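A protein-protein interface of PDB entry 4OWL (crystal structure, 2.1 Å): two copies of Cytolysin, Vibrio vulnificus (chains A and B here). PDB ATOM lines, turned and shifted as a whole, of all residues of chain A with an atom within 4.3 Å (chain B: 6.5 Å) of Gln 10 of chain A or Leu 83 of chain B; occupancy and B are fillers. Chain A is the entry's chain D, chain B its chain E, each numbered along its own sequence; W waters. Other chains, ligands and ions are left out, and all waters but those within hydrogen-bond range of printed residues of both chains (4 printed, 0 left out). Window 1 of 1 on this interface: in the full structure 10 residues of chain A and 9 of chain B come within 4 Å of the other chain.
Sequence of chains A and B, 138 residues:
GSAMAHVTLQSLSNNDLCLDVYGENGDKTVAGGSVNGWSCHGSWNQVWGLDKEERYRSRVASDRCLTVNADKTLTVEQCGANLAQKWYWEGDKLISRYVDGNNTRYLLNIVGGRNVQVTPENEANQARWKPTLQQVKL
The side-chain amide nitrogen (ND2) of Asn 15 of chain A is in hydrogen-bond range of the backbone carbonyl oxygen (O) of Val 99 of chain B (2.9 Å). O of Ala 81 of chain B sits at hydrogen-bond distance from NE2 of Gln 10 of chain A (2.8 Å). N of Leu 83 of chain B lies within hydrogen-bond range of O of Asn 15 of chain A (2.9 Å). The side-chain amide oxygen of Asn 82 of chain B sits close to the backbone carbonyl oxygen of Asn 15 of chain A, at 3.5 Å.
OG1 of Thr 132 of chain A is in hydrogen-bond range of O of Lys 130 of chain A (3.1 Å). OG of Ser 11 of chain A is in hydrogen-bond range of N of Asn 14 of chain A (3.1 Å). OG of Ser 96 of chain B sits at hydrogen-bond distance from N of Tyr 98 of chain B, at 2.9 Å. The backbone carbonyl oxygen (O) of Lys 86 of chain B is in hydrogen-bond range of the backbone NH (N) of Arg 97 of chain B (3.1 Å). The backbone NH (N) of Thr 8 of chain A sits at hydrogen-bond distance from the backbone carbonyl oxygen (O) of Thr 132 of chain A. The backbone NH (N) of Ser 11 of chain A sits at hydrogen-bond distance from the backbone carbonyl oxygen (O) of Leu 17 of chain A (2.9 Å).
Among the printed residues, merely in contact across the chains: Gln 10 of chain A with Leu 83 of chain B, Gln 10 of chain A with Lys 86 of chain B, Ser 11 of chain A with Leu 83 of chain B, Leu 12 of chain A with Leu 83 of chain B, Leu 12 of chain A with Arg 97 of chain B, Leu 12 of chain A with Val 99 of chain B, Asn 14 of chain A with Leu 83 of chain B, Asn 14 of chain A with Val 99 of chain B, Asn 15 of chain A with Tyr 98 of chain B, Cys 40 of chain A with Ala 81 of chain B and Thr 132 of chain A with Glu 53 of chain B.
Of chain A, only Gln 10, Ser 11, Leu 12, Asn 14 and Asn 15 come within 4 Å of Leu 83 of chain B. Of the printed residues of chain A, Lys 86 of chain B touches Gln 10. Of the printed residues of chain B, Ser 11 of chain A touches Leu 83. The nearest residue of chain B that does not touch Gln 10 of chain A is Asn 82 of chain B (4.8 Å). The nearest printed residue of chain A that does not touch Leu 83 of chain B is Leu 17 of chain A (6.5 Å). The nearest printed residue of chain B that does not touch Asn 15 of chain A is Arg 97 of chain B (4.3 Å).
Hydrophobic or aromatic side chains of chain B within 4 Å of the printed part of chain A: Ala 81, Leu 83, Tyr 98 and Val 99. Along chain B the printed residues that touch a printed residue of chain A span positions 53 to 99. Of the 13 printed residues of chain A, 7 touch a printed residue of chain B. Printed residues of chain A that touch a printed residue of chain B: Gln 10, Ser 11, Leu 12, Asn 14, Asn 15, Cys 40 and Thr 132. Hydrophobic or aromatic side chains of chain A within 4 Å of the printed part of chain B: Leu 12. Among the printed residues, 15 pairs touch across the chains.
No position is printed for both chains.
Water W4 lies within hydrogen-bond range of NZ of Lys 130 of chain A (2.6 Å), OE1 of Glu 53 of chain B (2.8 Å) and NZ of Lys 86 of chain B (3.2 Å). Water W3 lies within hydrogen-bond range of the backbone carbonyl oxygen of Leu 12 of chain A (2.7 Å) and the backbone carbonyl oxygen of Arg 97 of chain B (2.7 Å). Water W1 lies within hydrogen-bond range of the side-chain amino group (NZ) of Lys 86 of chain B and the side-chain amide oxygen (OE1) of Gln 10 of chain A. Water W2 bridges NZ of Lys 130 of chain A (3.1 Å) and OE1 of Glu 53 of chain B (3.3 Å).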
ATOM      1  N   THR A   8      37.143  16.811  21.493  1.00  0.00           N
ATOM      2  CA  THR A   8      36.114  15.962  22.066  1.00  0.00           C
ATOM      3  C   THR A   8      36.078  14.661  21.276  1.00  0.00           C
ATOM      4  O   THR A   8      36.496  14.611  20.124  1.00  0.00           O
ATOM      5  CB  THR A   8      34.766  16.641  22.042  1.00  0.00           C
ATOM      6  OG1 THR A   8      34.454  16.963  20.673  1.00  0.00           O
ATOM      7  CG2 THR A   8      34.797  17.962  22.891  1.00  0.00           C
ATOM      8  N   LEU A   9      35.585  13.586  21.897  1.00  0.00           N
ATOM      9  CA  LEU A   9      35.416  12.327  21.198  1.00  0.00           C
ATOM     10  C   LEU A   9      33.923  12.126  21.062  1.00  0.00           C
ATOM     11  O   LEU A   9      33.301  11.643  21.963  1.00  0.00           O
ATOM     12  CB  LEU A   9      36.095  11.177  21.962  1.00  0.00           C
ATOM     13  CG  LEU A   9      37.625  11.329  22.074  1.00  0.00           C
ATOM     14  CD1 LEU A   9      38.272  10.356  23.114  1.00  0.00           C
ATOM     15  CD2 LEU A   9      38.317  11.122  20.784  1.00  0.00           C
ATOM     16  N   GLN A  10      33.367  12.538  19.930  1.00  0.00           N
ATOM     17  CA  GLN A  10      31.938  12.472  19.688  1.00  0.00           C
ATOM     18  C   GLN A  10      31.558  11.202  18.887  1.00  0.00           C
ATOM     19  O   GLN A  10      32.155  10.886  17.862  1.00  0.00           O
ATOM     20  CB  GLN A  10      31.457  13.723  18.920  1.00  0.00           C
ATOM     21  CG  GLN A  10      29.909  13.780  18.863  1.00  0.00           C
ATOM     22  CD  GLN A  10      29.363  15.055  18.395  1.00  0.00           C
ATOM     23  OE1 GLN A  10      30.090  16.041  18.219  1.00  0.00           O
ATOM     24  NE2 GLN A  10      28.058  15.069  18.147  1.00  0.00           N
ATOM     25  N   SER A  11      30.519  10.522  19.346  1.00  0.00           N
ATOM     26  CA  SER A  11      29.966   9.374  18.611  1.00  0.00           C
ATOM     27  C   SER A  11      29.377   9.793  17.284  1.00  0.00           C
ATOM     28  O   SER A  11      28.690  10.822  17.192  1.00  0.00           O
ATOM     29  CB  SER A  11      28.900   8.684  19.473  1.00  0.00           C
ATOM     30  OG  SER A  11      28.273   7.640  18.809  1.00  0.00           O
ATOM     31  N   LEU A  12      29.627   8.997  16.249  1.00  0.00           N
ATOM     32  CA  LEU A  12      28.848   9.056  15.023  1.00  0.00           C
ATOM     33  C   LEU A  12      27.747   7.980  14.933  1.00  0.00           C
ATOM     34  O   LEU A  12      27.134   7.810  13.873  1.00  0.00           O
ATOM     35  CB  LEU A  12      29.781   8.906  13.806  1.00  0.00           C
ATOM     36  CG  LEU A  12      30.861  10.000  13.718  1.00  0.00           C
ATOM     37  CD1 LEU A  12      31.799   9.742  12.533  1.00  0.00           C
ATOM     38  CD2 LEU A  12      30.232  11.390  13.518  1.00  0.00           C
ATOM     39  N   ASN A  14      25.413   7.774  17.573  1.00  0.00           N
ATOM     40  CA  ASN A  14      24.360   8.270  18.443  1.00  0.00           C
ATOM     41  C   ASN A  14      24.275   9.797  18.139  1.00  0.00           C
ATOM     42  O   ASN A  14      25.334  10.443  18.012  1.00  0.00           O
ATOM     43  CB  ASN A  14      24.743   8.014  19.906  1.00  0.00           C
ATOM     44  CG  ASN A  14      23.749   8.578  20.903  1.00  0.00           C
ATOM     45  OD1 ASN A  14      23.481   9.818  20.983  1.00  0.00           O
ATOM     46  ND2 ASN A  14      23.247   7.672  21.778  1.00  0.00           N
ATOM     47  N   ASN A  15      23.057  10.352  18.046  1.00  0.00           N
ATOM     48  CA  ASN A  15      22.887  11.690  17.561  1.00  0.00           C
ATOM     49  C   ASN A  15      23.485  12.742  18.496  1.00  0.00           C
ATOM     50  O   ASN A  15      23.706  13.846  18.034  1.00  0.00           O
ATOM     51  CB  ASN A  15      21.416  12.004  17.320  1.00  0.00           C
ATOM     52  CG  ASN A  15      20.908  11.350  16.069  1.00  0.00           C
ATOM     53  OD1 ASN A  15      21.615  11.300  15.057  1.00  0.00           O
ATOM     54  ND2 ASN A  15      19.695  10.794  16.140  1.00  0.00           N
ATOM     55  N   LEU A  17      26.260  12.227  21.714  1.00  0.00           N
ATOM     56  CA  LEU A  17      26.982  11.527  22.757  1.00  0.00           C
ATOM     57  C   LEU A  17      28.468  11.799  22.580  1.00  0.00           C
ATOM     58  O   LEU A  17      28.976  11.618  21.490  1.00  0.00           O
ATOM     59  CB  LEU A  17      26.670  10.002  22.726  1.00  0.00           C
ATOM     60  CG  LEU A  17      27.222   9.298  23.968  1.00  0.00           C
ATOM     61  CD1 LEU A  17      26.401   8.059  24.339  1.00  0.00           C
ATOM     62  CD2 LEU A  17      28.684   8.892  23.826  1.00  0.00           C
ATOM     63  N   CYS A  18      29.108  12.331  23.632  1.00  0.00           N
ATOM     64  CA  CYS A  18      30.546  12.551  23.744  1.00  0.00           C
ATOM     65  C   CYS A  18      31.117  11.708  24.897  1.00  0.00           C
ATOM     66  O   CYS A  18      30.399  11.491  25.868  1.00  0.00           O
ATOM     67  CB  CYS A  18      30.845  14.093  24.054  1.00  0.00           C
ATOM     68  SG  CYS A  18      30.785  14.956  22.461  1.00  0.00           S
ATOM     69  N   CYS A  40      26.814  16.467  24.353  1.00  0.00           N
ATOM     70  CA  CYS A  40      28.093  17.131  24.115  1.00  0.00           C
ATOM     71  C   CYS A  40      28.007  18.579  24.593  1.00  0.00           C
ATOM     72  O   CYS A  40      27.065  19.266  24.260  1.00  0.00           O
ATOM     73  CB  CYS A  40      28.459  17.138  22.625  1.00  0.00           C
ATOM     74  SG  CYS A  40      28.844  15.507  21.944  1.00  0.00           S
ATOM     75  N   TRP A 129      33.407   6.987  15.951  1.00  0.00           N
ATOM     76  CA  TRP A 129      33.733   8.183  16.720  1.00  0.00           C
ATOM     77  C   TRP A 129      34.435   9.182  15.825  1.00  0.00           C
ATOM     78  O   TRP A 129      35.022   8.790  14.806  1.00  0.00           O
ATOM     79  CB  TRP A 129      34.637   7.820  17.901  1.00  0.00           C
ATOM     80  CG  TRP A 129      34.046   6.872  18.794  1.00  0.00           C
ATOM     81  CD1 TRP A 129      34.126   5.508  18.713  1.00  0.00           C
ATOM     82  CD2 TRP A 129      33.276   7.162  19.970  1.00  0.00           C
ATOM     83  NE1 TRP A 129      33.400   4.937  19.726  1.00  0.00           N
ATOM     84  CE2 TRP A 129      32.878   5.930  20.519  1.00  0.00           C
ATOM     85  CE3 TRP A 129      32.875   8.339  20.606  1.00  0.00           C
ATOM     86  CZ2 TRP A 129      32.086   5.854  21.666  1.00  0.00           C
ATOM     87  CZ3 TRP A 129      32.100   8.255  21.749  1.00  0.00           C
ATOM     88  CH2 TRP A 129      31.720   7.046  22.266  1.00  0.00           C
ATOM     89  N   LYS A 130      34.367  10.456  16.197  1.00  0.00           N
ATOM     90  CA  LYS A 130      35.008  11.562  15.450  1.00  0.00           C
ATOM     91  C   LYS A 130      35.789  12.359  16.501  1.00  0.00           C
ATOM     92  O   LYS A 130      35.194  12.914  17.403  1.00  0.00           O
ATOM     93  CB  LYS A 130      33.994  12.441  14.745  1.00  0.00           C
ATOM     94  CG  LYS A 130      34.608  13.602  13.965  1.00  0.00           C
ATOM     95  CD  LYS A 130      33.586  14.620  13.485  1.00  0.00           C
ATOM     96  CE  LYS A 130      34.248  15.855  12.828  1.00  0.00           C
ATOM     97  NZ  LYS A 130      33.181  16.899  12.474  1.00  0.00           N
ATOM     98  N   THR A 132      37.127  15.594  17.499  1.00  0.00           N
ATOM     99  CA  THR A 132      36.672  16.910  17.027  1.00  0.00           C
ATOM    100  C   THR A 132      37.520  17.977  17.743  1.00  0.00           C
ATOM    101  O   THR A 132      37.478  18.077  18.976  1.00  0.00           O
ATOM    102  CB  THR A 132      35.159  17.084  17.380  1.00  0.00           C
ATOM    103  OG1 THR A 132      34.415  15.890  17.002  1.00  0.00           O
ATOM    104  CG2 THR A 132      34.583  18.278  16.756  1.00  0.00           C
ATOM    105  N   GLU B  53      32.335  22.402  12.030  1.00  0.00           N
ATOM    106  CA  GLU B  53      31.655  21.279  12.713  1.00  0.00           C
ATOM    107  C   GLU B  53      30.752  20.531  11.766  1.00  0.00           C
ATOM    108  O   GLU B  53      29.949  19.733  12.215  1.00  0.00           O
ATOM    109  CB  GLU B  53      30.821  21.770  13.900  1.00  0.00           C
ATOM    110  CG  GLU B  53      31.612  22.597  14.922  1.00  0.00           C
ATOM    111  CD  GLU B  53      32.770  21.839  15.426  1.00  0.00           C
ATOM    112  OE1 GLU B  53      32.600  20.579  15.600  1.00  0.00           O
ATOM    113  OE2 GLU B  53      33.866  22.476  15.640  1.00  0.00           O
ATOM    114  N   VAL B  68      17.935  18.252  10.411  1.00  0.00           N
ATOM    115  CA  VAL B  68      17.013  17.154  10.161  1.00  0.00           C
ATOM    116  C   VAL B  68      16.118  16.950  11.353  1.00  0.00           C
ATOM    117  O   VAL B  68      16.577  16.844  12.475  1.00  0.00           O
ATOM    118  CB  VAL B  68      17.784  15.832   9.844  1.00  0.00           C
ATOM    119  CG1 VAL B  68      16.823  14.667   9.645  1.00  0.00           C
ATOM    120  CG2 VAL B  68      18.582  16.005   8.635  1.00  0.00           C
ATOM    121  N   ALA B  81      25.662  20.455  18.764  1.00  0.00           N
ATOM    122  CA  ALA B  81      26.490  19.307  18.460  1.00  0.00           C
ATOM    123  C   ALA B  81      25.740  18.152  17.795  1.00  0.00           C
ATOM    124  O   ALA B  81      26.355  17.161  17.349  1.00  0.00           O
ATOM    125  CB  ALA B  81      27.164  18.802  19.764  1.00  0.00           C
ATOM    126  N   ASN B  82      24.435  18.248  17.710  1.00  0.00           N
ATOM    127  CA  ASN B  82      23.643  17.088  17.254  1.00  0.00           C
ATOM    128  C   ASN B  82      24.064  16.639  15.847  1.00  0.00           C
ATOM    129  O   ASN B  82      24.303  17.473  14.922  1.00  0.00           O
ATOM    130  CB  ASN B  82      22.131  17.403  17.301  1.00  0.00           C
ATOM    131  CG  ASN B  82      21.261  16.093  17.441  1.00  0.00           C
ATOM    132  OD1 ASN B  82      21.031  15.412  16.457  1.00  0.00           O
ATOM    133  ND2 ASN B  82      20.847  15.753  18.649  1.00  0.00           N
ATOM    134  N   LEU B  83      24.140  15.327  15.631  1.00  0.00           N
ATOM    135  CA  LEU B  83      24.424  14.834  14.280  1.00  0.00           C
ATOM    136  C   LEU B  83      23.342  15.218  13.238  1.00  0.00           C
ATOM    137  O   LEU B  83      23.570  15.194  12.010  1.00  0.00           O
ATOM    138  CB  LEU B  83      24.582  13.306  14.302  1.00  0.00           C
ATOM    139  CG  LEU B  83      25.646  12.716  15.218  1.00  0.00           C
ATOM    140  CD1 LEU B  83      25.756  11.248  14.977  1.00  0.00           C
ATOM    141  CD2 LEU B  83      27.007  13.375  14.951  1.00  0.00           C
ATOM    142  N   ALA B  84      22.151  15.542  13.720  1.00  0.00           N
ATOM    143  CA  ALA B  84      21.045  15.997  12.850  1.00  0.00           C
ATOM    144  C   ALA B  84      21.381  17.349  12.138  1.00  0.00           C
ATOM    145  O   ALA B  84      20.704  17.775  11.165  1.00  0.00           O
ATOM    146  CB  ALA B  84      19.785  16.128  13.705  1.00  0.00           C
ATOM    147  N   GLN B  85      22.462  17.979  12.580  1.00  0.00           N
ATOM    148  CA  GLN B  85      22.943  19.251  11.987  1.00  0.00           C
ATOM    149  C   GLN B  85      24.230  19.090  11.205  1.00  0.00           C
ATOM    150  O   GLN B  85      24.837  20.082  10.804  1.00  0.00           O
ATOM    151  CB  GLN B  85      23.157  20.290  13.091  1.00  0.00           C
ATOM    152  CG  GLN B  85      21.888  20.731  13.682  1.00  0.00           C
ATOM    153  CD  GLN B  85      22.011  21.885  14.689  1.00  0.00           C
ATOM    154  OE1 GLN B  85      23.042  22.120  15.318  1.00  0.00           O
ATOM    155  NE2 GLN B  85      20.919  22.592  14.862  1.00  0.00           N
ATOM    156  N   LYS B  86      24.722  17.847  11.050  1.00  0.00           N
ATOM    157  CA  LYS B  86      26.014  17.659  10.409  1.00  0.00           C
ATOM    158  C   LYS B  86      25.781  17.094   9.030  1.00  0.00           C
ATOM    159  O   LYS B  86      24.925  16.223   8.860  1.00  0.00           O
ATOM    160  CB  LYS B  86      26.941  16.762  11.241  1.00  0.00           C
ATOM    161  CG  LYS B  86      27.312  17.363  12.579  1.00  0.00           C
ATOM    162  CD  LYS B  86      28.470  16.638  13.220  1.00  0.00           C
ATOM    163  CE  LYS B  86      28.684  17.064  14.639  1.00  0.00           C
ATOM    164  NZ  LYS B  86      28.883  18.555  14.743  1.00  0.00           N
ATOM    165  N   TRP B  87      26.595  17.542   8.065  1.00  0.00           N
ATOM    166  CA  TRP B  87      26.411  17.215   6.651  1.00  0.00           C
ATOM    167  C   TRP B  87      27.719  16.949   5.978  1.00  0.00           C
ATOM    168  O   TRP B  87      28.679  17.559   6.346  1.00  0.00           O
ATOM    169  CB  TRP B  87      25.714  18.344   5.921  1.00  0.00           C
ATOM    170  CG  TRP B  87      24.393  18.666   6.457  1.00  0.00           C
ATOM    171  CD1 TRP B  87      24.090  19.562   7.432  1.00  0.00           C
ATOM    172  CD2 TRP B  87      23.146  18.093   6.028  1.00  0.00           C
ATOM    173  NE1 TRP B  87      22.733  19.580   7.651  1.00  0.00           N
ATOM    174  CE2 TRP B  87      22.141  18.674   6.792  1.00  0.00           C
ATOM    175  CE3 TRP B  87      22.799  17.138   5.070  1.00  0.00           C
ATOM    176  CZ2 TRP B  87      20.836  18.330   6.650  1.00  0.00           C
ATOM    177  CZ3 TRP B  87      21.470  16.814   4.907  1.00  0.00           C
ATOM    178  CH2 TRP B  87      20.516  17.420   5.664  1.00  0.00           C
ATOM    179  N   SER B  96      23.341  13.430   5.406  1.00  0.00           N
ATOM    180  CA  SER B  96      23.218  13.753   6.822  1.00  0.00           C
ATOM    181  C   SER B  96      23.943  12.751   7.686  1.00  0.00           C
ATOM    182  O   SER B  96      24.047  11.610   7.299  1.00  0.00           O
ATOM    183  CB  SER B  96      21.754  13.748   7.194  1.00  0.00           C
ATOM    184  OG  SER B  96      21.588  13.918   8.567  1.00  0.00           O
ATOM    185  N   ARG B  97      24.475  13.167   8.819  1.00  0.00           N
ATOM    186  CA  ARG B  97      24.992  12.237   9.809  1.00  0.00           C
ATOM    187  C   ARG B  97      23.939  11.703  10.797  1.00  0.00           C
ATOM    188  O   ARG B  97      24.281  10.917  11.711  1.00  0.00           O
ATOM    189  CB  ARG B  97      26.115  12.877  10.593  1.00  0.00           C
ATOM    190  CG  ARG B  97      27.310  13.270   9.707  1.00  0.00           C
ATOM    191  CD  ARG B  97      28.579  13.136  10.432  1.00  0.00           C
ATOM    192  NE  ARG B  97      29.741  13.556   9.657  1.00  0.00           N
ATOM    193  CZ  ARG B  97      30.496  12.761   8.900  1.00  0.00           C
ATOM    194  NH1 ARG B  97      30.200  11.464   8.778  1.00  0.00           N
ATOM    195  NH2 ARG B  97      31.569  13.266   8.258  1.00  0.00           N
ATOM    196  N   TYR B  98      22.698  12.108  10.598  1.00  0.00           N
ATOM    197  CA  TYR B  98      21.595  11.691  11.443  1.00  0.00           C
ATOM    198  C   TYR B  98      21.515  10.163  11.514  1.00  0.00           C
ATOM    199  O   TYR B  98      21.634   9.524  10.466  1.00  0.00           O
ATOM    200  CB  TYR B  98      20.281  12.248  10.888  1.00  0.00           C
ATOM    201  CG  TYR B  98      19.082  11.821  11.665  1.00  0.00           C
ATOM    202  CD1 TYR B  98      18.763  12.430  12.870  1.00  0.00           C
ATOM    203  CD2 TYR B  98      18.234  10.886  11.167  1.00  0.00           C
ATOM    204  CE1 TYR B  98      17.641  12.000  13.628  1.00  0.00           C
ATOM    205  CE2 TYR B  98      17.099  10.477  11.879  1.00  0.00           C
ATOM    206  CZ  TYR B  98      16.811  11.063  13.099  1.00  0.00           C
ATOM    207  OH  TYR B  98      15.725  10.644  13.824  1.00  0.00           O
ATOM    208  N   VAL B  99      21.370   9.608  12.703  1.00  0.00           N
ATOM    209  CA  VAL B  99      21.191   8.197  12.872  1.00  0.00           C
ATOM    210  C   VAL B  99      19.822   7.882  13.467  1.00  0.00           C
ATOM    211  O   VAL B  99      19.279   8.607  14.282  1.00  0.00           O
ATOM    212  CB  VAL B  99      22.311   7.563  13.799  1.00  0.00           C
ATOM    213  CG1 VAL B  99      23.686   7.773  13.207  1.00  0.00           C
ATOM    214  CG2 VAL B  99      22.274   8.186  15.129  1.00  0.00           C
HETATM  215  O   HOH W   1      29.779  18.842  17.328  1.00  0.00           O
HETATM  216  O   HOH W   2      34.798  19.265  13.535  1.00  0.00           O
HETATM  217  O   HOH W   3      26.506   9.325  11.717  1.00  0.00           O
HETATM  218  O   HOH W   4      32.017  18.098  14.479  1.00  0.00           O
